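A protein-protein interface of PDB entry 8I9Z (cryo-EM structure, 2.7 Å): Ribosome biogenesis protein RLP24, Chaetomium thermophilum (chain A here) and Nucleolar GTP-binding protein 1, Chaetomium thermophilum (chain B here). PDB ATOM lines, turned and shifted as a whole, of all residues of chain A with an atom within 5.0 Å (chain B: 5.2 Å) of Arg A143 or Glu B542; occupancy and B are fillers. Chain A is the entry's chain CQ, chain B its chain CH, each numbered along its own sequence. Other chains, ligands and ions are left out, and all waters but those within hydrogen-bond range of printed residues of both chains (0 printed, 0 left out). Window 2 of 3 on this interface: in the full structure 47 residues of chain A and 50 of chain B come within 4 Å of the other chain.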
ATOM      1  N   GLY A 139     -10.552  23.320 -15.747  1.00  0.00           N
ATOM      2  CA  GLY A 139     -11.299  22.570 -14.723  1.00  0.00           C
ATOM      3  C   GLY A 139     -11.747  21.222 -15.240  1.00  0.00           C
ATOM      4  O   GLY A 139     -11.900  20.315 -14.417  1.00  0.00           O
ATOM      5  N   SER A 140     -11.926  21.092 -16.552  1.00  0.00           N
ATOM      6  CA  SER A 140     -12.315  19.803 -17.159  1.00  0.00           C
ATOM      7  C   SER A 140     -11.114  18.862 -17.128  1.00  0.00           C
ATOM      8  O   SER A 140     -11.324  17.648 -16.980  1.00  0.00           O
ATOM      9  CB  SER A 140     -12.795  20.011 -18.556  1.00  0.00           C
ATOM     10  OG  SER A 140     -11.769  20.572 -19.365  1.00  0.00           O
ATOM     11  N   GLU A 141      -9.906  19.408 -17.269  1.00  0.00           N
ATOM     12  CA  GLU A 141      -8.682  18.578 -17.193  1.00  0.00           C
ATOM     13  C   GLU A 141      -8.452  18.114 -15.757  1.00  0.00           C
ATOM     14  O   GLU A 141      -8.051  16.953 -15.589  1.00  0.00           O
ATOM     15  CB  GLU A 141      -7.463  19.358 -17.662  1.00  0.00           C
ATOM     16  CG  GLU A 141      -7.569  19.857 -19.089  1.00  0.00           C
ATOM     17  CD  GLU A 141      -6.427  20.754 -19.533  1.00  0.00           C
ATOM     18  OE1 GLU A 141      -5.736  21.314 -18.660  1.00  0.00           O
ATOM     19  OE2 GLU A 141      -6.232  20.892 -20.757  1.00  0.00           O
ATOM     20  N   LYS A 142      -8.703  18.971 -14.768  1.00  0.00           N
ATOM     21  CA  LYS A 142      -8.530  18.606 -13.340  1.00  0.00           C
ATOM     22  C   LYS A 142      -9.630  17.631 -12.963  1.00  0.00           C
ATOM     23  O   LYS A 142      -9.414  16.839 -12.039  1.00  0.00           O
ATOM     24  CB  LYS A 142      -8.624  19.828 -12.431  1.00  0.00           C
ATOM     25  CG  LYS A 142      -7.347  20.641 -12.300  1.00  0.00           C
ATOM     26  CD  LYS A 142      -7.519  21.851 -11.416  1.00  0.00           C
ATOM     27  CE  LYS A 142      -7.162  23.145 -12.112  1.00  0.00           C
ATOM     28  NZ  LYS A 142      -8.290  23.661 -12.922  1.00  0.00           N
ATOM     29  N   ARG A 143     -10.739  17.662 -13.689  1.00  0.00           N
ATOM     30  CA  ARG A 143     -11.832  16.706 -13.442  1.00  0.00           C
ATOM     31  C   ARG A 143     -11.416  15.348 -14.004  1.00  0.00           C
ATOM     32  O   ARG A 143     -11.575  14.345 -13.291  1.00  0.00           O
ATOM     33  CB  ARG A 143     -13.101  17.198 -14.133  1.00  0.00           C
ATOM     34  CG  ARG A 143     -14.379  16.924 -13.357  1.00  0.00           C
ATOM     35  CD  ARG A 143     -15.543  17.707 -13.929  1.00  0.00           C
ATOM     36  NE  ARG A 143     -16.360  18.293 -12.876  1.00  0.00           N
ATOM     37  CZ  ARG A 143     -16.671  19.580 -12.784  1.00  0.00           C
ATOM     38  NH1 ARG A 143     -16.239  20.438 -13.693  1.00  0.00           N
ATOM     39  NH2 ARG A 143     -17.422  20.003 -11.783  1.00  0.00           N
ATOM     40  N   ARG A 144     -10.924  15.323 -15.244  1.00  0.00           N
ATOM     41  CA  ARG A 144     -10.461  14.059 -15.857  1.00  0.00           C
ATOM     42  C   ARG A 144      -9.407  13.461 -14.939  1.00  0.00           C
ATOM     43  O   ARG A 144      -9.548  12.280 -14.571  1.00  0.00           O
ATOM     44  CB  ARG A 144      -9.896  14.306 -17.254  1.00  0.00           C
ATOM     45  CG  ARG A 144      -9.122  13.142 -17.853  1.00  0.00           C
ATOM     46  CD  ARG A 144      -8.106  13.615 -18.872  1.00  0.00           C
ATOM     47  NE  ARG A 144      -7.465  14.862 -18.481  1.00  0.00           N
ATOM     48  CZ  ARG A 144      -6.186  15.153 -18.687  1.00  0.00           C
ATOM     49  NH1 ARG A 144      -5.392  14.279 -19.282  1.00  0.00           N
ATOM     50  NH2 ARG A 144      -5.703  16.314 -18.290  1.00  0.00           N
ATOM     51  N   LEU A 145      -8.432  14.265 -14.537  1.00  0.00           N
ATOM     52  CA  LEU A 145      -7.325  13.731 -13.719  1.00  0.00           C
ATOM     53  C   LEU A 145      -7.803  13.385 -12.306  1.00  0.00           C
ATOM     54  O   LEU A 145      -7.074  12.637 -11.640  1.00  0.00           O
ATOM     55  CB  LEU A 145      -6.197  14.757 -13.694  1.00  0.00           C
ATOM     56  CG  LEU A 145      -5.261  14.726 -14.900  1.00  0.00           C
ATOM     57  CD1 LEU A 145      -3.856  15.125 -14.493  1.00  0.00           C
ATOM     58  CD2 LEU A 145      -5.246  13.352 -15.553  1.00  0.00           C
ATOM     59  N   ALA A 146      -8.964  13.868 -11.856  1.00  0.00           N
ATOM     60  CA  ALA A 146      -9.471  13.445 -10.525  1.00  0.00           C
ATOM     61  C   ALA A 146      -9.862  11.971 -10.597  1.00  0.00           C
ATOM     62  O   ALA A 146      -9.451  11.207  -9.701  1.00  0.00           O
ATOM     63  CB  ALA A 146     -10.634  14.289 -10.087  1.00  0.00           C
ATOM     64  N   GLU A 147     -10.619  11.589 -11.625  1.00  0.00           N
ATOM     65  CA  GLU A 147     -10.943  10.161 -11.830  1.00  0.00           C
ATOM     66  C   GLU A 147      -9.640   9.375 -11.949  1.00  0.00           C
ATOM     67  O   GLU A 147      -9.459   8.419 -11.177  1.00  0.00           O
ATOM     68  CB  GLU A 147     -11.746  10.018 -13.116  1.00  0.00           C
ATOM     69  CG  GLU A 147     -13.138  10.608 -13.023  1.00  0.00           C
ATOM     70  CD  GLU A 147     -13.425  11.741 -13.992  1.00  0.00           C
ATOM     71  OE1 GLU A 147     -12.917  11.690 -15.131  1.00  0.00           O
ATOM     72  OE2 GLU A 147     -14.160  12.672 -13.608  1.00  0.00           O
ATOM     73  N   ASP B 540     -14.601  24.798 -12.034  1.00  0.00           N
ATOM     74  CA  ASP B 540     -15.534  23.684 -12.295  1.00  0.00           C
ATOM     75  C   ASP B 540     -16.833  24.280 -12.815  1.00  0.00           C
ATOM     76  O   ASP B 540     -17.559  24.894 -12.023  1.00  0.00           O
ATOM     77  CB  ASP B 540     -15.756  22.884 -11.017  1.00  0.00           C
ATOM     78  CG  ASP B 540     -15.296  23.583  -9.747  1.00  0.00           C
ATOM     79  OD1 ASP B 540     -14.238  23.193  -9.217  1.00  0.00           O
ATOM     80  OD2 ASP B 540     -15.996  24.514  -9.303  1.00  0.00           O
ATOM     81  N   THR B 541     -17.113  24.089 -14.099  1.00  0.00           N
ATOM     82  CA  THR B 541     -18.319  24.686 -14.723  1.00  0.00           C
ATOM     83  C   THR B 541     -19.542  23.799 -14.466  1.00  0.00           C
ATOM     84  O   THR B 541     -20.666  24.289 -14.654  1.00  0.00           O
ATOM     85  CB  THR B 541     -18.087  24.935 -16.217  1.00  0.00           C
ATOM     86  OG1 THR B 541     -17.843  23.680 -16.854  1.00  0.00           O
ATOM     87  CG2 THR B 541     -16.932  25.875 -16.487  1.00  0.00           C
ATOM     88  N   GLU B 542     -19.328  22.552 -14.052  1.00  0.00           N
ATOM     89  CA  GLU B 542     -20.456  21.624 -13.807  1.00  0.00           C
ATOM     90  C   GLU B 542     -20.930  21.779 -12.363  1.00  0.00           C
ATOM     91  O   GLU B 542     -22.090  21.435 -12.092  1.00  0.00           O
ATOM     92  CB  GLU B 542     -20.038  20.193 -14.136  1.00  0.00           C
ATOM     93  CG  GLU B 542     -19.448  20.041 -15.525  1.00  0.00           C
ATOM     94  CD  GLU B 542     -20.309  20.578 -16.654  1.00  0.00           C
ATOM     95  OE1 GLU B 542     -21.394  20.011 -16.892  1.00  0.00           O
ATOM     96  OE2 GLU B 542     -19.891  21.562 -17.298  1.00  0.00           O
ATOM     97  N   ALA B 543     -20.076  22.290 -11.484  1.00  0.00           N
ATOM     98  CA  ALA B 543     -20.453  22.519 -10.076  1.00  0.00           C
ATOM     99  C   ALA B 543     -21.415  23.686  -9.980  1.00  0.00           C
ATOM    100  O   ALA B 543     -22.300  23.654  -9.111  1.00  0.00           O
ATOM    101  CB  ALA B 543     -19.225  22.853  -9.285  1.00  0.00           C
ATOM    102  N   ILE B 544     -21.239  24.680 -10.833  1.00  0.00           N
ATOM    103  CA  ILE B 544     -22.054  25.913 -10.730  1.00  0.00           C
ATOM    104  C   ILE B 544     -23.345  25.725 -11.520  1.00  0.00           C
ATOM    105  O   ILE B 544     -24.060  26.735 -11.776  1.00  0.00           O
ATOM    106  CB  ILE B 544     -21.195  27.082 -11.242  1.00  0.00           C
ATOM    107  CG1 ILE B 544     -21.045  27.084 -12.764  1.00  0.00           C
ATOM    108  CG2 ILE B 544     -19.830  27.048 -10.579  1.00  0.00           C
ATOM    109  CD1 ILE B 544     -20.399  28.333 -13.315  1.00  0.00           C
ATOM    110  N   GLY B 545     -23.655  24.493 -11.903  1.00  0.00           N
ATOM    111  CA  GLY B 545     -24.840  24.271 -12.744  1.00  0.00           C
ATOM    112  C   GLY B 545     -25.006  25.420 -13.711  1.00  0.00           C
ATOM    113  O   GLY B 545     -26.090  26.025 -13.711  1.00  0.00           O
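OE2 of Glu B542 sits at hydrogen-bond distance from OG1 of Thr B541, at 3.0 Å.
Among the printed residues, merely in contact across the chains: Arg A143 with Asp B540 (3.4 Å), Arg A143 with Thr B541 (3.8 Å), Arg A143 with Glu B542 (3.5 Å) and Arg A143 with Ala B543 (3.5 Å).
Of chain B, only Asp B540 (3.4 Å), Thr B541 (3.8 Å), Glu B542 (3.5 Å) and Ala B543 (3.5 Å) come within 4 Å of Arg A143.
Of the printed residues of chain A, Asp B540 touches Arg A143 (3.4 Å).
Printed residues of chain A within 4 Å of Ala B543: Arg A143 (3.5 Å).
Printed residues of chain A within 4 Å of Thr B541: Arg A143 (3.8 Å).
The nearest printed residue of chain A that does not touch Glu B542 is Ser A140 (7.3 Å).
The nearest printed residue of chain A that does not touch Ala B543 is Gly A139 (8.9 Å).
Of the 6 printed residues of chain B, 4 touch a printed residue of chain A.
Printed residues of chain B that touch a printed residue of chain A: Asp B540, Thr B541, Glu B542 and Ala B543.
Among the printed residues, 4 pairs touch across the chains.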
